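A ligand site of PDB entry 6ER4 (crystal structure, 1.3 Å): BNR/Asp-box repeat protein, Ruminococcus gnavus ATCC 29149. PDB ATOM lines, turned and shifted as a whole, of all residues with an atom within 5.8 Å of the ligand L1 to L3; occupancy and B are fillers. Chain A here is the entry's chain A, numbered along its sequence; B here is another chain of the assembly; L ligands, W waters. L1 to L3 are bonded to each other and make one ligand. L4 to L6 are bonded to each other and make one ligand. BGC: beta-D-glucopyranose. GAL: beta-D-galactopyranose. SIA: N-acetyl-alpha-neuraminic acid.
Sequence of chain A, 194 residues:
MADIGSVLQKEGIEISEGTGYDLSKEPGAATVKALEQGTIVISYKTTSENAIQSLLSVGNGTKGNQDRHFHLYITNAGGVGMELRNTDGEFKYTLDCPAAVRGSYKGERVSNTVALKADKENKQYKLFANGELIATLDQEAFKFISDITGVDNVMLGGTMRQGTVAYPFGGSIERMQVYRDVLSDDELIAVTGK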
ATOM      1  N   ILE A  52      -7.005  -1.989   0.844  1.00  0.00           N
ATOM      2  CA  ILE A  52      -5.673  -2.606   0.676  1.00  0.00           C
ATOM      3  C   ILE A  52      -5.410  -3.460   1.925  1.00  0.00           C
ATOM      4  O   ILE A  52      -5.362  -2.934   3.032  1.00  0.00           O
ATOM      5  CB  ILE A  52      -4.554  -1.555   0.512  1.00  0.00           C
ATOM      6  CG1 ILE A  52      -4.852  -0.570  -0.613  1.00  0.00           C
ATOM      7  CG2 ILE A  52      -3.247  -2.270   0.266  1.00  0.00           C
ATOM      8  CD1 ILE A  52      -4.022   0.693  -0.488  1.00  0.00           C
ATOM      9  N   GLN A  66       8.808   4.376   6.887  1.00  0.00           N
ATOM     10  CA  GLN A  66       7.509   3.870   6.456  1.00  0.00           C
ATOM     11  C   GLN A  66       7.425   3.473   4.984  1.00  0.00           C
ATOM     12  O   GLN A  66       6.453   2.835   4.589  1.00  0.00           O
ATOM     13  CB  GLN A  66       6.377   4.883   6.762  1.00  0.00           C
ATOM     14  CG  GLN A  66       6.536   6.264   6.122  1.00  0.00           C
ATOM     15  CD  GLN A  66       7.337   7.268   6.920  1.00  0.00           C
ATOM     16  OE1 GLN A  66       8.100   6.917   7.795  1.00  0.00           O
ATOM     17  NE2 GLN A  66       7.159   8.527   6.604  1.00  0.00           N
ATOM     18  N   ASP A  67       8.395   3.868   4.166  1.00  0.00           N
ATOM     19  CA  ASP A  67       8.441   3.454   2.762  1.00  0.00           C
ATOM     20  C   ASP A  67       9.452   2.363   2.502  1.00  0.00           C
ATOM     21  O   ASP A  67       9.796   2.136   1.336  1.00  0.00           O
ATOM     22  CB  ASP A  67       8.686   4.668   1.830  1.00  0.00           C
ATOM     23  CG  ASP A  67       7.629   5.735   1.915  1.00  0.00           C
ATOM     24  OD1 ASP A  67       6.502   5.478   2.357  1.00  0.00           O
ATOM     25  OD2 ASP A  67       7.943   6.870   1.466  1.00  0.00           O
ATOM     26  N   HIS A  71       5.233  -6.002   0.653  1.00  0.00           N
ATOM     27  CA  HIS A  71       4.012  -6.756   0.999  1.00  0.00           C
ATOM     28  C   HIS A  71       3.315  -7.314  -0.209  1.00  0.00           C
ATOM     29  O   HIS A  71       3.452  -6.805  -1.327  1.00  0.00           O
ATOM     30  CB  HIS A  71       3.043  -5.917   1.857  1.00  0.00           C
ATOM     31  CG  HIS A  71       2.382  -4.778   1.139  1.00  0.00           C
ATOM     32  ND1 HIS A  71       1.019  -4.537   1.218  1.00  0.00           N
ATOM     33  CD2 HIS A  71       2.898  -3.776   0.376  1.00  0.00           C
ATOM     34  CE1 HIS A  71       0.733  -3.441   0.567  1.00  0.00           C
ATOM     35  NE2 HIS A  71       1.846  -2.961   0.032  1.00  0.00           N
ATOM     36  N   TYR A  73      -0.547  -8.225  -1.214  1.00  0.00           N
ATOM     37  CA  TYR A  73      -1.831  -7.707  -0.733  1.00  0.00           C
ATOM     38  C   TYR A  73      -2.978  -8.073  -1.679  1.00  0.00           C
ATOM     39  O   TYR A  73      -2.755  -8.410  -2.840  1.00  0.00           O
ATOM     40  CB  TYR A  73      -1.791  -6.199  -0.521  1.00  0.00           C
ATOM     41  CG  TYR A  73      -1.658  -5.369  -1.757  1.00  0.00           C
ATOM     42  CD1 TYR A  73      -2.789  -4.990  -2.490  1.00  0.00           C
ATOM     43  CD2 TYR A  73      -0.423  -4.965  -2.239  1.00  0.00           C
ATOM     44  CE1 TYR A  73      -2.691  -4.210  -3.621  1.00  0.00           C
ATOM     45  CE2 TYR A  73      -0.335  -4.176  -3.370  1.00  0.00           C
ATOM     46  CZ  TYR A  73      -1.451  -3.810  -4.053  1.00  0.00           C
ATOM     47  OH  TYR A  73      -1.325  -3.032  -5.172  1.00  0.00           O
ATOM     48  N   GLU A  83       3.944  -4.702  -3.385  1.00  0.00           N
ATOM     49  CA  GLU A  83       4.866  -3.575  -3.477  1.00  0.00           C
ATOM     50  C   GLU A  83       6.168  -3.976  -2.813  1.00  0.00           C
ATOM     51  O   GLU A  83       6.180  -4.567  -1.731  1.00  0.00           O
ATOM     52  CB  GLU A  83       4.347  -2.326  -2.831  1.00  0.00           C
ATOM     53  CG  GLU A  83       2.973  -1.886  -3.256  1.00  0.00           C
ATOM     54  CD  GLU A  83       2.615  -0.567  -2.614  1.00  0.00           C
ATOM     55  OE1 GLU A  83       2.201  -0.549  -1.423  1.00  0.00           O
ATOM     56  OE2 GLU A  83       2.784   0.483  -3.288  1.00  0.00           O
ATOM     57  N   ARG A  85       9.617  -1.944  -1.742  1.00  0.00           N
ATOM     58  CA  ARG A  85       9.952  -0.522  -1.553  1.00  0.00           C
ATOM     59  C   ARG A  85      11.128  -0.307  -0.633  1.00  0.00           C
ATOM     60  O   ARG A  85      11.244  -0.977   0.413  1.00  0.00           O
ATOM     61  CB  ARG A  85       8.756   0.190  -0.937  1.00  0.00           C
ATOM     62  CG  ARG A  85       7.498   0.088  -1.764  1.00  0.00           C
ATOM     63  CD  ARG A  85       6.389   1.020  -1.284  1.00  0.00           C
ATOM     64  NE  ARG A  85       6.821   2.416  -1.420  1.00  0.00           N
ATOM     65  CZ  ARG A  85       6.131   3.458  -0.930  1.00  0.00           C
ATOM     66  NH1 ARG A  85       5.012   3.270  -0.227  1.00  0.00           N
ATOM     67  NH2 ARG A  85       6.585   4.684  -1.103  1.00  0.00           N
ATOM     68  N   ASP A  88      11.189   5.825  -2.457  1.00  0.00           N
ATOM     69  CA  ASP A  88      11.027   5.931  -3.916  1.00  0.00           C
ATOM     70  C   ASP A  88      12.321   6.323  -4.635  1.00  0.00           C
ATOM     71  O   ASP A  88      12.503   5.976  -5.767  1.00  0.00           O
ATOM     72  CB  ASP A  88       9.883   6.894  -4.258  1.00  0.00           C
ATOM     73  CG  ASP A  88       8.513   6.426  -3.781  1.00  0.00           C
ATOM     74  OD1 ASP A  88       8.377   5.267  -3.366  1.00  0.00           O
ATOM     75  OD2 ASP A  88       7.596   7.247  -3.831  1.00  0.00           O
ATOM     76  N   GLY A  89      13.188   7.029  -3.931  1.00  0.00           N
ATOM     77  CA  GLY A  89      14.508   7.375  -4.464  1.00  0.00           C
ATOM     78  C   GLY A  89      15.416   6.182  -4.708  1.00  0.00           C
ATOM     79  O   GLY A  89      16.330   6.260  -5.525  1.00  0.00           O
ATOM     80  N   LYS A  92      10.788   1.468  -6.109  1.00  0.00           N
ATOM     81  CA  LYS A  92       9.370   1.173  -5.845  1.00  0.00           C
ATOM     82  C   LYS A  92       8.852   0.299  -6.959  1.00  0.00           C
ATOM     83  O   LYS A  92       8.540   0.760  -8.050  1.00  0.00           O
ATOM     84  CB  LYS A  92       8.555   2.462  -5.771  1.00  0.00           C
ATOM     85  CG  LYS A  92       7.121   2.187  -5.355  1.00  0.00           C
ATOM     86  CD  LYS A  92       6.261   3.430  -5.322  1.00  0.00           C
ATOM     87  CE  LYS A  92       4.897   3.061  -4.755  1.00  0.00           C
ATOM     88  NZ  LYS A  92       3.992   4.238  -4.736  1.00  0.00           N
ATOM     89  N   THR A  94       6.144  -2.510  -8.196  1.00  0.00           N
ATOM     90  CA  THR A  94       4.778  -2.868  -7.829  1.00  0.00           C
ATOM     91  C   THR A  94       4.086  -3.647  -8.924  1.00  0.00           C
ATOM     92  O   THR A  94       4.425  -3.549 -10.107  1.00  0.00           O
ATOM     93  CB  THR A  94       3.947  -1.607  -7.531  1.00  0.00           C
ATOM     94  OG1 THR A  94       3.676  -0.929  -8.736  1.00  0.00           O
ATOM     95  CG2 THR A  94       4.589  -0.693  -6.551  1.00  0.00           C
ATOM     96  N   ASP A  96      -0.242  -4.731  -9.629  1.00  0.00           N
ATOM     97  CA  ASP A  96      -1.638  -4.608  -9.237  1.00  0.00           C
ATOM     98  C   ASP A  96      -2.478  -5.176 -10.360  1.00  0.00           C
ATOM     99  O   ASP A  96      -2.413  -4.690 -11.499  1.00  0.00           O
ATOM    100  CB  ASP A  96      -1.995  -3.153  -8.961  1.00  0.00           C
ATOM    101  CG  ASP A  96      -3.162  -3.044  -8.119  1.00  0.00           C
ATOM    102  OD1 ASP A  96      -4.247  -3.122  -8.701  1.00  0.00           O
ATOM    103  OD2 ASP A  96      -3.015  -2.983  -6.867  1.00  0.00           O
ATOM    104  N   ARG A 161       4.242   0.348   9.754  1.00  0.00           N
ATOM    105  CA  ARG A 161       4.693   1.647   9.251  1.00  0.00           C
ATOM    106  C   ARG A 161       4.728   2.573  10.464  1.00  0.00           C
ATOM    107  O   ARG A 161       3.682   2.942  11.000  1.00  0.00           O
ATOM    108  CB  ARG A 161       3.769   2.168   8.168  1.00  0.00           C
ATOM    109  CG  ARG A 161       3.620   1.188   6.990  1.00  0.00           C
ATOM    110  CD  ARG A 161       2.834   1.793   5.829  1.00  0.00           C
ATOM    111  NE  ARG A 161       3.658   2.682   5.042  1.00  0.00           N
ATOM    112  CZ  ARG A 161       3.209   3.411   4.047  1.00  0.00           C
ATOM    113  NH1 ARG A 161       1.920   3.524   3.843  1.00  0.00           N
ATOM    114  NH2 ARG A 161       4.058   4.107   3.300  1.00  0.00           N
ATOM    115  N   TYR A 167      -2.497  -1.045   6.013  1.00  0.00           N
ATOM    116  CA  TYR A 167      -3.029  -1.989   5.004  1.00  0.00           C
ATOM    117  C   TYR A 167      -3.695  -3.206   5.678  1.00  0.00           C
ATOM    118  O   TYR A 167      -3.338  -4.359   5.449  1.00  0.00           O
ATOM    119  CB  TYR A 167      -1.964  -2.447   4.022  1.00  0.00           C
ATOM    120  CG  TYR A 167      -1.168  -1.331   3.349  1.00  0.00           C
ATOM    121  CD1 TYR A 167      -1.776  -0.179   2.878  1.00  0.00           C
ATOM    122  CD2 TYR A 167       0.188  -1.443   3.182  1.00  0.00           C
ATOM    123  CE1 TYR A 167      -1.034   0.815   2.220  1.00  0.00           C
ATOM    124  CE2 TYR A 167       0.941  -0.478   2.537  1.00  0.00           C
ATOM    125  CZ  TYR A 167       0.337   0.668   2.073  1.00  0.00           C
ATOM    126  OH  TYR A 167       1.040   1.621   1.390  1.00  0.00           O
ATOM    127  N   ALA B  51       9.215  16.804  -8.510  1.00  0.00           N
ATOM    128  CA  ALA B  51       9.393  15.385  -8.183  1.00  0.00           C
ATOM    129  C   ALA B  51       8.942  14.428  -9.289  1.00  0.00           C
ATOM    130  O   ALA B  51       9.610  13.442  -9.583  1.00  0.00           O
ATOM    131  CB  ALA B  51       8.663  15.061  -6.897  1.00  0.00           C
ATOM    132  N   ILE B  52       7.767  14.698  -9.876  1.00  0.00           N
ATOM    133  CA  ILE B  52       7.175  13.844 -10.892  1.00  0.00           C
ATOM    134  C   ILE B  52       6.819  14.739 -12.057  1.00  0.00           C
ATOM    135  O   ILE B  52       6.004  15.680 -11.913  1.00  0.00           O
ATOM    136  CB  ILE B  52       5.920  13.131 -10.410  1.00  0.00           C
ATOM    137  CG1 ILE B  52       6.193  12.329  -9.125  1.00  0.00           C
ATOM    138  CG2 ILE B  52       5.341  12.225 -11.502  1.00  0.00           C
ATOM    139  CD1 ILE B  52       4.917  11.975  -8.399  1.00  0.00           C
ATOM    140  N   ASP B  88      -8.628   2.737  -9.722  1.00  0.00           N
ATOM    141  CA  ASP B  88      -7.933   1.542  -9.250  1.00  0.00           C
ATOM    142  C   ASP B  88      -8.794   0.270  -9.280  1.00  0.00           C
ATOM    143  O   ASP B  88      -8.281  -0.803  -9.419  1.00  0.00           O
ATOM    144  CB  ASP B  88      -7.343   1.790  -7.868  1.00  0.00           C
ATOM    145  CG  ASP B  88      -6.270   2.864  -7.835  1.00  0.00           C
ATOM    146  OD1 ASP B  88      -5.804   3.314  -8.874  1.00  0.00           O
ATOM    147  OD2 ASP B  88      -5.902   3.239  -6.703  1.00  0.00           O
ATOM    148  N   LYS B  92      -4.734  -0.287 -12.618  1.00  0.00           N
ATOM    149  CA  LYS B  92      -3.619   0.610 -12.331  1.00  0.00           C
ATOM    150  C   LYS B  92      -2.349  -0.136 -12.652  1.00  0.00           C
ATOM    151  O   LYS B  92      -1.865  -0.937 -11.845  1.00  0.00           O
ATOM    152  CB  LYS B  92      -3.613   1.058 -10.872  1.00  0.00           C
ATOM    153  CG  LYS B  92      -2.565   2.126 -10.606  1.00  0.00           C
ATOM    154  CD  LYS B  92      -2.466   2.595  -9.196  1.00  0.00           C
ATOM    155  CE  LYS B  92      -1.476   3.749  -9.094  1.00  0.00           C
ATOM    156  NZ  LYS B  92      -1.323   4.222  -7.683  1.00  0.00           N
HETATM  157  C2  BGC L   1       5.800  10.163  -3.586  1.00  0.00           C
HETATM  158  C3  BGC L   1       4.771  10.834  -2.676  1.00  0.00           C
HETATM  159  C4  BGC L   1       4.957  10.300  -1.267  1.00  0.00           C
HETATM  160  C5  BGC L   1       6.423  10.532  -0.856  1.00  0.00           C
HETATM  161  C6  BGC L   1       6.734  10.003   0.558  1.00  0.00           C
HETATM  162  C1  BGC L   1       7.210  10.404  -3.052  1.00  0.00           C
HETATM  163  O1  BGC L   1       8.159   9.698  -3.848  1.00  0.00           O
HETATM  164  O2  BGC L   1       5.650  10.747  -4.890  1.00  0.00           O
HETATM  165  O3  BGC L   1       3.460  10.562  -3.191  1.00  0.00           O
HETATM  166  O4  BGC L   1       4.093  11.072  -0.437  1.00  0.00           O
HETATM  167  O5  BGC L   1       7.244   9.794  -1.761  1.00  0.00           O
HETATM  168  O6  BGC L   1       6.257   8.666   0.752  1.00  0.00           O
HETATM  169  C1  GAL L   2       3.397  10.309   0.533  1.00  0.00           C
HETATM  170  C2  GAL L   2       2.812  11.287   1.543  1.00  0.00           C
HETATM  171  C3  GAL L   2       1.978  10.529   2.580  1.00  0.00           C
HETATM  172  C4  GAL L   2       0.949   9.670   1.871  1.00  0.00           C
HETATM  173  C5  GAL L   2       1.646   8.792   0.824  1.00  0.00           C
HETATM  174  C6  GAL L   2       0.627   7.962   0.078  1.00  0.00           C
HETATM  175  O2  GAL L   2       3.868  11.951   2.234  1.00  0.00           O
HETATM  176  O3  GAL L   2       1.354  11.433   3.468  1.00  0.00           O
HETATM  177  O4  GAL L   2       0.005  10.487   1.163  1.00  0.00           O
HETATM  178  O5  GAL L   2       2.378   9.612  -0.120  1.00  0.00           O
HETATM  179  O6  GAL L   2       1.302   7.087  -0.843  1.00  0.00           O
HETATM  180  C1  SIA L   3       1.830   5.414   0.790  1.00  0.00           C
HETATM  181  C2  SIA L   3       1.256   5.692  -0.583  1.00  0.00           C
HETATM  182  C3  SIA L   3       1.998   4.984  -1.741  1.00  0.00           C
HETATM  183  C4  SIA L   3       1.708   3.494  -1.730  1.00  0.00           C
HETATM  184  C5  SIA L   3       0.194   3.222  -1.743  1.00  0.00           C
HETATM  185  C6  SIA L   3      -0.416   3.944  -0.535  1.00  0.00           C
HETATM  186  C7  SIA L   3      -1.929   3.829  -0.380  1.00  0.00           C
HETATM  187  C8  SIA L   3      -2.437   4.711   0.760  1.00  0.00           C
HETATM  188  C9  SIA L   3      -3.866   4.337   1.094  1.00  0.00           C
HETATM  189  C10 SIA L   3      -0.928   1.181  -2.442  1.00  0.00           C
HETATM  190  C11 SIA L   3      -0.934  -0.313  -2.396  1.00  0.00           C
HETATM  191  N5  SIA L   3      -0.045   1.774  -1.699  1.00  0.00           N
HETATM  192  O1A SIA L   3       3.083   5.312   0.925  1.00  0.00           O
HETATM  193  O1B SIA L   3       1.047   5.324   1.762  1.00  0.00           O
HETATM  194  O4  SIA L   3       2.305   2.980  -2.918  1.00  0.00           O
HETATM  195  O6  SIA L   3      -0.132   5.352  -0.649  1.00  0.00           O
HETATM  196  O7  SIA L   3      -2.587   4.190  -1.584  1.00  0.00           O
HETATM  197  O8  SIA L   3      -1.607   4.600   1.945  1.00  0.00           O
HETATM  198  O9  SIA L   3      -4.446   5.324   1.940  1.00  0.00           O
HETATM  199  O10 SIA L   3      -1.754   1.827  -3.116  1.00  0.00           O
HETATM  200  C2  BGC L   4      -6.047   4.376  -3.395  1.00  0.00           C
HETATM  201  C3  BGC L   4      -5.969   5.676  -2.631  1.00  0.00           C
HETATM  202  C4  BGC L   4      -6.429   6.808  -3.535  1.00  0.00           C
HETATM  203  C5  BGC L   4      -7.830   6.507  -4.038  1.00  0.00           C
HETATM  204  C6  BGC L   4      -8.411   7.587  -4.944  1.00  0.00           C
HETATM  205  C1  BGC L   4      -7.454   4.177  -3.938  1.00  0.00           C
HETATM  206  O1  BGC L   4      -7.573   3.014  -4.736  1.00  0.00           O
HETATM  207  O2  BGC L   4      -5.682   3.318  -2.519  1.00  0.00           O
HETATM  208  O3  BGC L   4      -4.623   5.909  -2.209  1.00  0.00           O
HETATM  209  O4  BGC L   4      -6.493   7.979  -2.728  1.00  0.00           O
HETATM  210  O5  BGC L   4      -7.764   5.272  -4.773  1.00  0.00           O
HETATM  211  O6  BGC L   4      -7.505   7.959  -5.982  1.00  0.00           O
HETATM  212  C1  GAL L   5      -5.936   9.186  -3.168  1.00  0.00           C
HETATM  213  C2  GAL L   5      -6.470  10.431  -2.503  1.00  0.00           C
HETATM  214  C3  GAL L   5      -5.850  11.685  -3.094  1.00  0.00           C
HETATM  215  C4  GAL L   5      -4.341  11.527  -3.228  1.00  0.00           C
HETATM  216  C5  GAL L   5      -4.016  10.259  -3.992  1.00  0.00           C
HETATM  217  C6  GAL L   5      -2.505  10.102  -4.141  1.00  0.00           C
HETATM  218  O2  GAL L   5      -7.902  10.448  -2.566  1.00  0.00           O
HETATM  219  O3  GAL L   5      -6.185  12.778  -2.214  1.00  0.00           O
HETATM  220  O4  GAL L   5      -3.729  11.404  -1.934  1.00  0.00           O
HETATM  221  O5  GAL L   5      -4.533   9.100  -3.340  1.00  0.00           O
HETATM  222  O6  GAL L   5      -2.248   8.925  -4.948  1.00  0.00           O
HETATM  223  C1  SIA L   6      -2.532  10.112  -7.021  1.00  0.00           C
HETATM  224  C2  SIA L   6      -1.639   9.189  -6.202  1.00  0.00           C
HETATM  225  C3  SIA L   6      -1.375   7.846  -6.839  1.00  0.00           C
HETATM  226  C4  SIA L   6      -0.446   7.953  -8.046  1.00  0.00           C
HETATM  227  C5  SIA L   6       0.846   8.669  -7.681  1.00  0.00           C
HETATM  228  C6  SIA L   6       0.456  10.034  -7.096  1.00  0.00           C
HETATM  229  C7  SIA L   6       1.654  10.890  -6.636  1.00  0.00           C
HETATM  230  C8  SIA L   6       1.168  12.148  -5.876  1.00  0.00           C
HETATM  231  C9  SIA L   6       2.286  13.140  -5.751  1.00  0.00           C
HETATM  232  C10 SIA L   6       2.966   8.636  -8.875  1.00  0.00           C
HETATM  233  C11 SIA L   6       3.661   8.652 -10.221  1.00  0.00           C
HETATM  234  N5  SIA L   6       1.656   8.817  -8.873  1.00  0.00           N
HETATM  235  O1A SIA L   6      -3.500   9.628  -7.643  1.00  0.00           O
HETATM  236  O1B SIA L   6      -2.277  11.347  -7.021  1.00  0.00           O
HETATM  237  O4  SIA L   6      -0.177   6.604  -8.453  1.00  0.00           O
HETATM  238  O6  SIA L   6      -0.373   9.807  -5.915  1.00  0.00           O
HETATM  239  O7  SIA L   6       2.486  10.131  -5.722  1.00  0.00           O
HETATM  240  O8  SIA L   6       0.092  12.752  -6.584  1.00  0.00           O
HETATM  241  O9  SIA L   6       1.880  14.164  -4.831  1.00  0.00           O
HETATM  242  O10 SIA L   6       3.570   8.524  -7.817  1.00  0.00           O
HETATM  243  O   HOH W   1       4.790   7.472   3.141  1.00  0.00           O
HETATM  244  O   HOH W   2       2.263   7.020   3.891  1.00  0.00           O
HETATM  245  O   HOH W   3       4.817   6.902  -0.526  1.00  0.00           O
HETATM  246  O   HOH W   4       0.718   8.630  -3.483  1.00  0.00           O
HETATM  247  O   HOH W   5      -5.080   7.358   0.252  1.00  0.00           O
HETATM  248  O   HOH W   6      -1.705   4.746  -4.526  1.00  0.00           O
HETATM  249  O   HOH W   7       6.369  13.264  -5.150  1.00  0.00           O
HETATM  250  O   HOH W   8       5.547  13.826   1.000  1.00  0.00           O
HETATM  251  O   HOH W   9      -1.493   6.989  -2.605  1.00  0.00           O
HETATM  252  O   HOH W  10       9.405   7.394  -0.802  1.00  0.00           O
HETATM  253  O   HOH W  11      -0.787   2.184  -5.887  1.00  0.00           O
HETATM  254  O   HOH W  12       5.511  10.129   3.997  1.00  0.00           O
HETATM  255  O   HOH W  13       0.455  11.211  -1.769  1.00  0.00           O
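Water W3 lies within hydrogen-bond range of O6 of BGC L1 (2.6 Å) and NH2 of Arg 85 (2.9 Å). Water W5 lies within hydrogen-bond range of an oxygen (O9) of SIA L3 and an oxygen (O3) of BGC L4. Water W2 bridges O1B of SIA L3 (3.0 Å) and NH2 of Arg 161 (3.5 Å). Water W1 lies within hydrogen-bond range of the side-chain carboxylate (OD1) of Asp 67 (2.7 Å), an oxygen (O6) of BGC L1 (3.0 Å) and the guanidinium group (NH2) of Arg 161 (3.4 Å). Water W4 lies within hydrogen-bond range of an oxygen (O6) of SIA L6 and an oxygen (O6) of GAL L2. Water W6 bridges an oxygen (O7) of SIA L3 (3.1 Å) and the side-chain amino group of Lys 92 of chain B (3.2 Å).
O7 of SIA L3 lies within hydrogen-bond range of O3 of BGC L4 (2.7 Å).
The side-chain carboxylate (OD2) of Asp 88 of chain A sits at hydrogen-bond distance from an oxygen (O1) of BGC L1, at 2.5 Å. The side-chain carboxylate of Asp 67 sits at hydrogen-bond distance from an oxygen (O6) of BGC L1, at 2.6 Å. The side-chain carboxylate of Glu 83 sits at hydrogen-bond distance from an oxygen (O4) of SIA L3, 2.6 Å away. O4 of SIA L3 is in hydrogen-bond range of NZ of Lys 92 of chain A (2.8 Å). NH2 of Arg 161 is in salt-bridge range of O1A of SIA L3, at 2.8 Å. The guanidinium group (NH1) of Arg 85 lies within salt-bridge range of an oxygen (O1A) of SIA L3 (3.0 Å). A nitrogen (N5) of SIA L3 lies within hydrogen-bond range of the side-chain hydroxyl (OH) of Tyr 167, at 3.3 Å. The side-chain amino group (NZ) of Lys 92 of chain B sits at hydrogen-bond distance from an oxygen (O4) of SIA L6. The side-chain carboxylate (OD2) of Asp 88 of chain B sits at hydrogen-bond distance from an oxygen (O1) of BGC L4 (2.6 Å).
The guanidinium group of Arg 85 lies within salt-bridge range of the side-chain carboxylate of Asp 88 of chain A, at 2.9 Å. NH2 of Arg 161 lies within salt-bridge range of OD1 of Asp 67 (3.0 Å). The side-chain carboxylate of Asp 67 is in salt-bridge range of the guanidinium group of Arg 85. OE1 of Glu 83 is in hydrogen-bond range of NE2 of His 71, at 2.8 Å. NH1 of Arg 161 sits at hydrogen-bond distance from OH of Tyr 167 (3.2 Å). O of Gln 66 lies within hydrogen-bond range of NE of Arg 161 (2.8 Å).
CD1 of Ile 52 of chain A touches O10 of SIA L3, at 3.7 Å. CZ of Tyr 73 touches C11 of SIA L3, 3.9 Å away. Ile 52 of chain B touches the ligand L1 to L3. Hydrophobic or aromatic side chains within 4 Å of the ligand L1 to L3: Ile 52 of chain A, Tyr 73, Tyr 167 and Ile 52 of chain B. Along chain A the residues within 4 Å of the ligand L1 to L3 span positions 52 to 167.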
